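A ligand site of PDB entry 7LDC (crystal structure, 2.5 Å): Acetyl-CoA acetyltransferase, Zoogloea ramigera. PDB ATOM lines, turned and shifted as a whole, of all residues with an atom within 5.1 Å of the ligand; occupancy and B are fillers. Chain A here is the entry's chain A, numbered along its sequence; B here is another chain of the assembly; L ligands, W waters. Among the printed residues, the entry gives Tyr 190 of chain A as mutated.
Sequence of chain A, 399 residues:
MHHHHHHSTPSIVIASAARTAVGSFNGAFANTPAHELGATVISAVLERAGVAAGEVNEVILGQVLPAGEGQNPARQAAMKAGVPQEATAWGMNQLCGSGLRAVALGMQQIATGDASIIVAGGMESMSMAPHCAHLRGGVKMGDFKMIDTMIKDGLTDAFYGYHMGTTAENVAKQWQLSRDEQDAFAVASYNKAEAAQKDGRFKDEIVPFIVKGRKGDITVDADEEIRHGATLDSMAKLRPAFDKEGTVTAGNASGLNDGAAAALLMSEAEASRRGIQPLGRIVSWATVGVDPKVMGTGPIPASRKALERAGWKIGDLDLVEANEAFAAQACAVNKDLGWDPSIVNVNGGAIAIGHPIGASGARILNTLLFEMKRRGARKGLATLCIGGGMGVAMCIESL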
ATOM      1  N   SCY A  96      17.599 -12.437  -0.354  1.00  0.00           N
ATOM      2  CA  SCY A  96      18.346 -11.749  -1.379  1.00  0.00           C
ATOM      3  CB  SCY A  96      17.479 -10.744  -2.091  1.00  0.00           C
ATOM      4  SG  SCY A  96      16.173 -11.563  -3.001  1.00  0.00           S
ATOM      5  CD  SCY A  96      14.798 -11.555  -1.988  1.00  0.00           C
ATOM      6  OCD SCY A  96      14.511 -10.733  -1.106  1.00  0.00           O
ATOM      7  CE  SCY A  96      13.900 -12.710  -2.312  1.00  0.00           C
ATOM      8  C   SCY A  96      19.641 -10.989  -0.894  1.00  0.00           C
ATOM      9  O   SCY A  96      20.469 -10.577  -1.746  1.00  0.00           O
ATOM     10  N   LEU A 155      10.421 -16.888  -3.173  1.00  0.00           N
ATOM     11  CA  LEU A 155       9.752 -15.823  -3.901  1.00  0.00           C
ATOM     12  C   LEU A 155       8.354 -15.494  -3.380  1.00  0.00           C
ATOM     13  O   LEU A 155       7.692 -14.632  -3.957  1.00  0.00           O
ATOM     14  CB  LEU A 155       9.649 -16.196  -5.393  1.00  0.00           C
ATOM     15  CG  LEU A 155      10.965 -16.592  -6.078  1.00  0.00           C
ATOM     16  CD1 LEU A 155      10.734 -16.891  -7.545  1.00  0.00           C
ATOM     17  CD2 LEU A 155      12.024 -15.513  -5.897  1.00  0.00           C
ATOM     18  N   HIS A 163       3.375 -13.097  -4.371  1.00  0.00           N
ATOM     19  CA  HIS A 163       4.735 -13.129  -4.880  1.00  0.00           C
ATOM     20  C   HIS A 163       5.457 -11.829  -4.543  1.00  0.00           C
ATOM     21  O   HIS A 163       4.852 -10.818  -4.188  1.00  0.00           O
ATOM     22  CB  HIS A 163       4.719 -13.349  -6.391  1.00  0.00           C
ATOM     23  CG  HIS A 163       5.998 -13.862  -6.959  1.00  0.00           C
ATOM     24  ND1 HIS A 163       7.074 -13.038  -7.252  1.00  0.00           N
ATOM     25  CD2 HIS A 163       6.388 -15.115  -7.307  1.00  0.00           C
ATOM     26  CE1 HIS A 163       8.056 -13.769  -7.742  1.00  0.00           C
ATOM     27  NE2 HIS A 163       7.667 -15.023  -7.794  1.00  0.00           N
ATOM     28  N   MET A 164       6.794 -11.868  -4.663  1.00  0.00           N
ATOM     29  CA  MET A 164       7.588 -10.662  -4.522  1.00  0.00           C
ATOM     30  C   MET A 164       7.223  -9.620  -5.581  1.00  0.00           C
ATOM     31  O   MET A 164       7.375  -8.415  -5.333  1.00  0.00           O
ATOM     32  CB  MET A 164       9.082 -11.000  -4.615  1.00  0.00           C
ATOM     33  CG  MET A 164       9.661 -11.750  -3.420  1.00  0.00           C
ATOM     34  SD  MET A 164       9.510 -10.845  -1.866  1.00  0.00           S
ATOM     35  CE  MET A 164       8.115 -11.674  -1.104  1.00  0.00           C
ATOM     36  N   TYR A 190      19.373  -2.888 -19.599  1.00  0.00           N
ATOM     37  CA  TYR A 190      19.866  -3.800 -20.624  1.00  0.00           C
ATOM     38  C   TYR A 190      20.965  -3.160 -21.472  1.00  0.00           C
ATOM     39  O   TYR A 190      21.978  -3.790 -21.781  1.00  0.00           O
ATOM     40  CB  TYR A 190      18.716  -4.261 -21.512  1.00  0.00           C
ATOM     41  CG  TYR A 190      17.854  -5.358 -20.927  1.00  0.00           C
ATOM     42  CD1 TYR A 190      18.292  -6.679 -20.897  1.00  0.00           C
ATOM     43  CD2 TYR A 190      16.591  -5.068 -20.399  1.00  0.00           C
ATOM     44  CE1 TYR A 190      17.496  -7.677 -20.357  1.00  0.00           C
ATOM     45  CE2 TYR A 190      15.809  -6.061 -19.862  1.00  0.00           C
ATOM     46  CZ  TYR A 190      16.255  -7.368 -19.839  1.00  0.00           C
ATOM     47  OH  TYR A 190      15.472  -8.361 -19.302  1.00  0.00           O
ATOM     48  N   ARG A 227      20.308  -9.886 -22.979  1.00  0.00           N
ATOM     49  CA  ARG A 227      19.789  -9.998 -24.349  1.00  0.00           C
ATOM     50  C   ARG A 227      20.225  -8.772 -25.147  1.00  0.00           C
ATOM     51  O   ARG A 227      20.104  -7.633 -24.678  1.00  0.00           O
ATOM     52  CB  ARG A 227      18.260 -10.154 -24.355  1.00  0.00           C
ATOM     53  CG  ARG A 227      17.469  -8.956 -23.824  1.00  0.00           C
ATOM     54  CD  ARG A 227      15.952  -9.162 -23.881  1.00  0.00           C
ATOM     55  NE  ARG A 227      15.488 -10.432 -23.321  1.00  0.00           N
ATOM     56  CZ  ARG A 227      14.826 -11.359 -24.011  1.00  0.00           C
ATOM     57  NH1 ARG A 227      14.437 -12.483 -23.427  1.00  0.00           N
ATOM     58  NH2 ARG A 227      14.542 -11.154 -25.284  1.00  0.00           N
ATOM     59  N   SER A 234       8.992  -3.946 -27.862  1.00  0.00           N
ATOM     60  CA  SER A 234       8.772  -5.312 -27.381  1.00  0.00           C
ATOM     61  C   SER A 234       8.601  -5.352 -25.876  1.00  0.00           C
ATOM     62  O   SER A 234       7.923  -6.230 -25.351  1.00  0.00           O
ATOM     63  CB  SER A 234       9.918  -6.222 -27.824  1.00  0.00           C
ATOM     64  OG  SER A 234      10.037  -6.254 -29.232  1.00  0.00           O
ATOM     65  N   MET A 235       9.224  -4.399 -25.170  1.00  0.00           N
ATOM     66  CA  MET A 235       9.057  -4.326 -23.714  1.00  0.00           C
ATOM     67  C   MET A 235       7.640  -3.928 -23.339  1.00  0.00           C
ATOM     68  O   MET A 235       7.070  -4.454 -22.375  1.00  0.00           O
ATOM     69  CB  MET A 235      10.070  -3.337 -23.131  1.00  0.00           C
ATOM     70  CG  MET A 235      10.078  -3.266 -21.624  1.00  0.00           C
ATOM     71  SD  MET A 235      10.889  -4.684 -20.862  1.00  0.00           S
ATOM     72  CE  MET A 235      12.532  -4.531 -21.554  1.00  0.00           C
ATOM     73  N   LEU A 238       4.576  -6.697 -23.558  1.00  0.00           N
ATOM     74  CA  LEU A 238       4.478  -7.812 -22.627  1.00  0.00           C
ATOM     75  C   LEU A 238       3.316  -7.610 -21.658  1.00  0.00           C
ATOM     76  O   LEU A 238       2.947  -6.481 -21.319  1.00  0.00           O
ATOM     77  CB  LEU A 238       5.784  -7.969 -21.853  1.00  0.00           C
ATOM     78  CG  LEU A 238       7.041  -8.206 -22.690  1.00  0.00           C
ATOM     79  CD1 LEU A 238       8.277  -8.262 -21.815  1.00  0.00           C
ATOM     80  CD2 LEU A 238       6.903  -9.493 -23.487  1.00  0.00           C
ATOM     81  N   ALA A 241       2.905  -9.910 -15.122  1.00  0.00           N
ATOM     82  CA  ALA A 241       3.197 -11.264 -14.679  1.00  0.00           C
ATOM     83  C   ALA A 241       2.621 -11.607 -13.305  1.00  0.00           C
ATOM     84  O   ALA A 241       2.594 -12.784 -12.941  1.00  0.00           O
ATOM     85  CB  ALA A 241       4.707 -11.499 -14.660  1.00  0.00           C
ATOM     86  N   PHE A 242       2.177 -10.614 -12.531  1.00  0.00           N
ATOM     87  CA  PHE A 242       1.688 -10.854 -11.171  1.00  0.00           C
ATOM     88  C   PHE A 242       0.299 -10.295 -10.897  1.00  0.00           C
ATOM     89  O   PHE A 242      -0.373 -10.814 -10.000  1.00  0.00           O
ATOM     90  CB  PHE A 242       2.669 -10.279 -10.136  1.00  0.00           C
ATOM     91  CG  PHE A 242       4.093 -10.700 -10.366  1.00  0.00           C
ATOM     92  CD1 PHE A 242       4.563 -11.900  -9.872  1.00  0.00           C
ATOM     93  CD2 PHE A 242       4.961  -9.888 -11.064  1.00  0.00           C
ATOM     94  CE1 PHE A 242       5.870 -12.291 -10.076  1.00  0.00           C
ATOM     95  CE2 PHE A 242       6.277 -10.266 -11.275  1.00  0.00           C
ATOM     96  CZ  PHE A 242       6.734 -11.472 -10.778  1.00  0.00           C
ATOM     97  N   THR A 249       6.109  -6.700 -15.260  1.00  0.00           N
ATOM     98  CA  THR A 249       6.120  -7.770 -16.259  1.00  0.00           C
ATOM     99  C   THR A 249       7.425  -8.549 -16.163  1.00  0.00           C
ATOM    100  O   THR A 249       8.317  -8.224 -15.372  1.00  0.00           O
ATOM    101  CB  THR A 249       5.975  -7.189 -17.677  1.00  0.00           C
ATOM    102  OG1 THR A 249       7.140  -6.420 -17.991  1.00  0.00           O
ATOM    103  CG2 THR A 249       4.742  -6.299 -17.761  1.00  0.00           C
ATOM    104  N   ALA A 250       7.535  -9.590 -16.993  1.00  0.00           N
ATOM    105  CA  ALA A 250       8.765 -10.372 -17.047  1.00  0.00           C
ATOM    106  C   ALA A 250       9.932  -9.551 -17.595  1.00  0.00           C
ATOM    107  O   ALA A 250      11.091  -9.891 -17.328  1.00  0.00           O
ATOM    108  CB  ALA A 250       8.562 -11.622 -17.894  1.00  0.00           C
ATOM    109  N   GLY A 251       9.652  -8.488 -18.335  1.00  0.00           N
ATOM    110  CA  GLY A 251      10.694  -7.671 -18.929  1.00  0.00           C
ATOM    111  C   GLY A 251      11.292  -6.653 -17.967  1.00  0.00           C
ATOM    112  O   GLY A 251      12.507  -6.442 -17.969  1.00  0.00           O
ATOM    113  N   ALA A 253      11.271  -6.914 -14.712  1.00  0.00           N
ATOM    114  CA  ALA A 253      11.584  -7.579 -13.456  1.00  0.00           C
ATOM    115  C   ALA A 253      12.774  -8.505 -13.666  1.00  0.00           C
ATOM    116  O   ALA A 253      13.004  -9.003 -14.773  1.00  0.00           O
ATOM    117  CB  ALA A 253      10.393  -8.390 -12.931  1.00  0.00           C
ATOM    118  N   SER A 254      13.542  -8.715 -12.603  1.00  0.00           N
ATOM    119  CA  SER A 254      14.642  -9.651 -12.664  1.00  0.00           C
ATOM    120  C   SER A 254      14.109 -11.070 -12.815  1.00  0.00           C
ATOM    121  O   SER A 254      12.958 -11.371 -12.487  1.00  0.00           O
ATOM    122  CB  SER A 254      15.535  -9.544 -11.427  1.00  0.00           C
ATOM    123  OG  SER A 254      14.814  -9.830 -10.233  1.00  0.00           O
ATOM    124  N   GLY A 255      14.960 -11.962 -13.325  1.00  0.00           N
ATOM    125  CA  GLY A 255      14.587 -13.323 -13.608  1.00  0.00           C
ATOM    126  C   GLY A 255      15.116 -14.307 -12.582  1.00  0.00           C
ATOM    127  O   GLY A 255      15.652 -13.945 -11.536  1.00  0.00           O
ATOM    128  N   LEU A 256      14.952 -15.588 -12.901  1.00  0.00           N
ATOM    129  CA  LEU A 256      15.447 -16.680 -12.083  1.00  0.00           C
ATOM    130  C   LEU A 256      16.782 -17.143 -12.662  1.00  0.00           C
ATOM    131  O   LEU A 256      16.888 -17.411 -13.852  1.00  0.00           O
ATOM    132  CB  LEU A 256      14.442 -17.839 -12.083  1.00  0.00           C
ATOM    133  CG  LEU A 256      12.973 -17.418 -11.963  1.00  0.00           C
ATOM    134  CD1 LEU A 256      12.054 -18.615 -12.124  1.00  0.00           C
ATOM    135  CD2 LEU A 256      12.722 -16.726 -10.626  1.00  0.00           C
ATOM    136  N   MET A 295       8.701  -4.433   0.485  1.00  0.00           N
ATOM    137  CA  MET A 295      10.045  -4.869   0.809  1.00  0.00           C
ATOM    138  C   MET A 295      11.107  -4.259  -0.097  1.00  0.00           C
ATOM    139  O   MET A 295      12.294  -4.255   0.265  1.00  0.00           O
ATOM    140  CB  MET A 295      10.138  -6.393   0.751  1.00  0.00           C
ATOM    141  CG  MET A 295       9.954  -6.970  -0.643  1.00  0.00           C
ATOM    142  SD  MET A 295      11.505  -7.202  -1.524  1.00  0.00           S
ATOM    143  CE  MET A 295      10.936  -7.127  -3.220  1.00  0.00           C
ATOM    144  N   ALA A 325      16.008  -5.618  -8.241  1.00  0.00           N
ATOM    145  CA  ALA A 325      15.033  -6.703  -8.127  1.00  0.00           C
ATOM    146  C   ALA A 325      13.846  -6.454  -9.047  1.00  0.00           C
ATOM    147  O   ALA A 325      13.406  -7.352  -9.783  1.00  0.00           O
ATOM    148  CB  ALA A 325      14.579  -6.856  -6.677  1.00  0.00           C
ATOM    149  N   PHE A 326      13.313  -5.235  -9.030  1.00  0.00           N
ATOM    150  CA  PHE A 326      12.230  -4.821  -9.901  1.00  0.00           C
ATOM    151  C   PHE A 326      12.457  -3.385 -10.316  1.00  0.00           C
ATOM    152  O   PHE A 326      13.119  -2.616  -9.607  1.00  0.00           O
ATOM    153  CB  PHE A 326      10.862  -4.968  -9.232  1.00  0.00           C
ATOM    154  CG  PHE A 326      10.522  -6.389  -8.840  1.00  0.00           C
ATOM    155  CD1 PHE A 326       9.862  -7.221  -9.716  1.00  0.00           C
ATOM    156  CD2 PHE A 326      10.853  -6.871  -7.575  1.00  0.00           C
ATOM    157  CE1 PHE A 326       9.539  -8.515  -9.364  1.00  0.00           C
ATOM    158  CE2 PHE A 326      10.534  -8.173  -7.218  1.00  0.00           C
ATOM    159  CZ  PHE A 326       9.876  -8.999  -8.107  1.00  0.00           C
ATOM    160  N   HIS A 355      19.449 -12.456 -11.403  1.00  0.00           N
ATOM    161  CA  HIS A 355      19.264 -12.309  -9.958  1.00  0.00           C
ATOM    162  C   HIS A 355      19.274 -13.671  -9.296  1.00  0.00           C
ATOM    163  O   HIS A 355      18.226 -14.214  -8.927  1.00  0.00           O
ATOM    164  CB  HIS A 355      17.957 -11.561  -9.659  1.00  0.00           C
ATOM    165  CG  HIS A 355      17.815 -11.106  -8.236  1.00  0.00           C
ATOM    166  ND1 HIS A 355      18.610 -11.597  -7.212  1.00  0.00           N
ATOM    167  CD2 HIS A 355      16.979 -10.223  -7.671  1.00  0.00           C
ATOM    168  CE1 HIS A 355      18.258 -11.019  -6.076  1.00  0.00           C
ATOM    169  NE2 HIS A 355      17.269 -10.173  -6.325  1.00  0.00           N
ATOM    170  N   ILE A 357      19.329 -15.403  -6.146  1.00  0.00           N
ATOM    171  CA  ILE A 357      18.952 -14.794  -4.874  1.00  0.00           C
ATOM    172  C   ILE A 357      20.071 -14.907  -3.840  1.00  0.00           C
ATOM    173  O   ILE A 357      20.505 -13.900  -3.258  1.00  0.00           O
ATOM    174  CB  ILE A 357      17.626 -15.387  -4.360  1.00  0.00           C
ATOM    175  CG1 ILE A 357      17.581 -16.891  -4.601  1.00  0.00           C
ATOM    176  CG2 ILE A 357      16.454 -14.713  -5.043  1.00  0.00           C
ATOM    177  CD1 ILE A 357      16.290 -17.531  -4.131  1.00  0.00           C
ATOM    178  N   CYS A 385      17.559  -5.046  -1.580  1.00  0.00           N
ATOM    179  CA  CYS A 385      16.339  -5.284  -0.833  1.00  0.00           C
ATOM    180  C   CYS A 385      16.213  -6.761  -0.512  1.00  0.00           C
ATOM    181  O   CYS A 385      16.808  -7.618  -1.178  1.00  0.00           O
ATOM    182  CB  CYS A 385      15.112  -4.802  -1.612  1.00  0.00           C
ATOM    183  SG  CYS A 385      14.866  -5.605  -3.214  1.00  0.00           S
ATOM    184  N   LYS B 140       8.246 -26.797 -15.094  1.00  0.00           N
ATOM    185  CA  LYS B 140       9.225 -25.713 -15.150  1.00  0.00           C
ATOM    186  C   LYS B 140       9.153 -24.829 -13.915  1.00  0.00           C
ATOM    187  O   LYS B 140      10.192 -24.429 -13.365  1.00  0.00           O
ATOM    188  CB  LYS B 140       9.007 -24.867 -16.407  1.00  0.00           C
ATOM    189  CG  LYS B 140       9.820 -23.583 -16.433  1.00  0.00           C
ATOM    190  CD  LYS B 140       9.427 -22.694 -17.610  1.00  0.00           C
ATOM    191  CE  LYS B 140      10.150 -21.363 -17.561  1.00  0.00           C
ATOM    192  NZ  LYS B 140       9.739 -20.457 -18.675  1.00  0.00           N
ATOM    193  N   MET B 141       7.948 -24.518 -13.447  1.00  0.00           N
ATOM    194  CA  MET B 141       7.772 -23.584 -12.353  1.00  0.00           C
ATOM    195  C   MET B 141       6.368 -23.725 -11.771  1.00  0.00           C
ATOM    196  O   MET B 141       5.407 -23.906 -12.518  1.00  0.00           O
ATOM    197  CB  MET B 141       8.018 -22.150 -12.831  1.00  0.00           C
ATOM    198  CG  MET B 141       7.911 -21.083 -11.771  1.00  0.00           C
ATOM    199  SD  MET B 141       8.276 -19.470 -12.487  1.00  0.00           S
ATOM    200  CE  MET B 141       6.935 -19.304 -13.660  1.00  0.00           C
HETATM  201  N1  LIG L   1      12.391  -7.876 -23.537  1.00  0.00           N
HETATM  202  C1  LIG L   1      11.537  -8.376 -24.437  1.00  0.00           C
HETATM  203  N2  LIG L   1      10.841  -9.491 -24.242  1.00  0.00           N
HETATM  204  C2  LIG L   1      10.990 -10.177 -23.106  1.00  0.00           C
HETATM  205  C3  LIG L   1      11.883  -9.683 -22.143  1.00  0.00           C
HETATM  206  C4  LIG L   1      12.585  -8.511 -22.379  1.00  0.00           C
HETATM  207  N3  LIG L   1      13.445  -8.083 -21.412  1.00  0.00           N
HETATM  208  N4  LIG L   1      11.888 -10.506 -21.082  1.00  0.00           N
HETATM  209  C5  LIG L   1      11.068 -11.473 -21.315  1.00  0.00           C
HETATM  210  N5  LIG L   1      10.479 -11.320 -22.549  1.00  0.00           N
HETATM  211  C6  LIG L   1       9.500 -12.278 -23.090  1.00  0.00           C
HETATM  212  C7  LIG L   1      10.129 -13.708 -23.158  1.00  0.00           C
HETATM  213  O1  LIG L   1      10.889 -14.005 -24.347  1.00  0.00           O
HETATM  214  C8  LIG L   1       8.848 -14.574 -23.089  1.00  0.00           C
HETATM  215  O2  LIG L   1       8.138 -14.548 -24.337  1.00  0.00           O
HETATM  216  P1  LIG L   1       7.779 -16.059 -24.795  1.00  0.00           P
HETATM  217  O3  LIG L   1       6.991 -16.728 -23.742  1.00  0.00           O
HETATM  218  O4  LIG L   1       6.882 -15.950 -26.142  1.00  0.00           O
HETATM  219  O5  LIG L   1       9.131 -16.898 -25.071  1.00  0.00           O
HETATM  220  C9  LIG L   1       8.067 -13.818 -21.998  1.00  0.00           C
HETATM  221  O6  LIG L   1       8.390 -12.439 -22.169  1.00  0.00           O
HETATM  222  C10 LIG L   1       8.490 -14.271 -20.598  1.00  0.00           C
HETATM  223  O7  LIG L   1       9.000 -15.593 -20.637  1.00  0.00           O
HETATM  224  P2  LIG L   1       9.831 -15.885 -19.277  1.00  0.00           P
HETATM  225  O8  LIG L   1      11.104 -15.132 -19.313  1.00  0.00           O
HETATM  226  O9  LIG L   1      10.151 -17.483 -19.214  1.00  0.00           O
HETATM  227  O10 LIG L   1       8.991 -15.372 -17.981  1.00  0.00           O
HETATM  228  P3  LIG L   1       8.828 -16.516 -16.848  1.00  0.00           P
HETATM  229  O11 LIG L   1       7.860 -17.511 -17.335  1.00  0.00           O
HETATM  230  O12 LIG L   1      10.241 -17.247 -16.538  1.00  0.00           O
HETATM  231  O13 LIG L   1       8.245 -15.859 -15.484  1.00  0.00           O
HETATM  232  C11 LIG L   1       8.597 -14.022 -13.955  1.00  0.00           C
HETATM  233  C12 LIG L   1       8.624 -14.483 -15.413  1.00  0.00           C
HETATM  234  C13 LIG L   1       8.651 -12.496 -13.899  1.00  0.00           C
HETATM  235  C14 LIG L   1       7.288 -14.476 -13.292  1.00  0.00           C
HETATM  236  C15 LIG L   1       9.823 -14.624 -13.246  1.00  0.00           C
HETATM  237  O14 LIG L   1      10.992 -14.152 -13.902  1.00  0.00           O
HETATM  238  C16 LIG L   1       9.901 -14.277 -11.773  1.00  0.00           C
HETATM  239  O15 LIG L   1       9.323 -14.964 -10.961  1.00  0.00           O
HETATM  240  N6  LIG L   1      10.642 -13.237 -11.349  1.00  0.00           N
HETATM  241  C17 LIG L   1      10.715 -12.931  -9.918  1.00  0.00           C
HETATM  242  C18 LIG L   1      12.093 -12.366  -9.552  1.00  0.00           C
HETATM  243  C19 LIG L   1      12.264 -12.281  -8.062  1.00  0.00           C
HETATM  244  O16 LIG L   1      11.303 -12.439  -7.332  1.00  0.00           O
HETATM  245  N7  LIG L   1      13.469 -12.023  -7.535  1.00  0.00           N
HETATM  246  C20 LIG L   1      13.627 -11.942  -6.083  1.00  0.00           C
HETATM  247  C21 LIG L   1      13.987 -10.510  -5.670  1.00  0.00           C
HETATM  248  S1  LIG L   1      12.790  -9.928  -4.449  1.00  0.00           S
HETATM  249  O   HOH W   1      13.939 -11.475 -19.362  1.00  0.00           O
HETATM  250  O   HOH W   2      11.653 -11.632 -15.196  1.00  0.00           O
HETATM  251  O   HOH W   3      15.134 -14.148  -8.971  1.00  0.00           O
HETATM  252  O   HOH W   4      13.309 -15.985 -15.360  1.00  0.00           O
HETATM  253  O   HOH W   5       5.605 -15.030 -16.735  1.00  0.00           O
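A nitrogen (N3) of the ligand lies within hydrogen-bond range of the side-chain hydroxyl (OH) of Tyr 190, 2.9 Å away. NZ of Lys 140 of chain B is in salt-bridge range of O9 of the ligand (3.1 Å). O of Ser 254 lies within hydrogen-bond range of N6 of the ligand, 3.2 Å away.
Merely in contact with the ligand: His 355 (3.4 Å), Leu 155 (3.5 Å), His 163 (3.5 Å), Leu 238 (3.6 Å), SCY 96 (3.6 Å), Met 295 (3.6 Å), Arg 227 (3.6 Å), Met 235 (3.7 Å), Gly 255 (3.7 Å), Gly 251 (3.7 Å), Met 164 (3.8 Å), Ala 250 (3.8 Å), Phe 242 (3.8 Å), Phe 326 (3.8 Å), Ala 325 (3.8 Å) and Leu 256 (3.8 Å). Hydrophobic or aromatic side chains that line the ligand: Leu 155, His 163, Met 164, Tyr 190, Met 235, Leu 238, Phe 242, Ala 250, Leu 256, Met 295, Ala 325, Phe 326 and His 355. Of the 26 residues printed, 19 come within 4 Å of the ligand. The nearest printed residue that does not touch the ligand is Ile 357 (4.1 Å).
Water W1 lies within hydrogen-bond range of a nitrogen (N4) of the ligand and the side-chain hydroxyl of Tyr 190. Water W3 lies within hydrogen-bond range of the backbone carbonyl oxygen of Gly 255 (2.6 Å), a nitrogen (N7) of the ligand (3.1 Å) and the backbone carbonyl oxygen of His 355 (3.1 Å). Water W4 bridges the backbone NH of Leu 256 and an oxygen (O14) of the ligand.
The backbone carbonyl oxygen (O) of Leu 155 lies within hydrogen-bond range of the backbone NH (N) of Met 164, at 3.0 Å. The backbone NH of Gly 251 lies close to the side-chain hydroxyl of Thr 249 (3.3 Å). A ring nitrogen (NE2) of His 355 lies close to SG of SCY 96, at 3.8 Å. The backbone carbonyl oxygen (O) of Ala 325 sits at hydrogen-bond distance from the side-chain hydroxyl (OG) of Ser 254 (2.9 Å).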
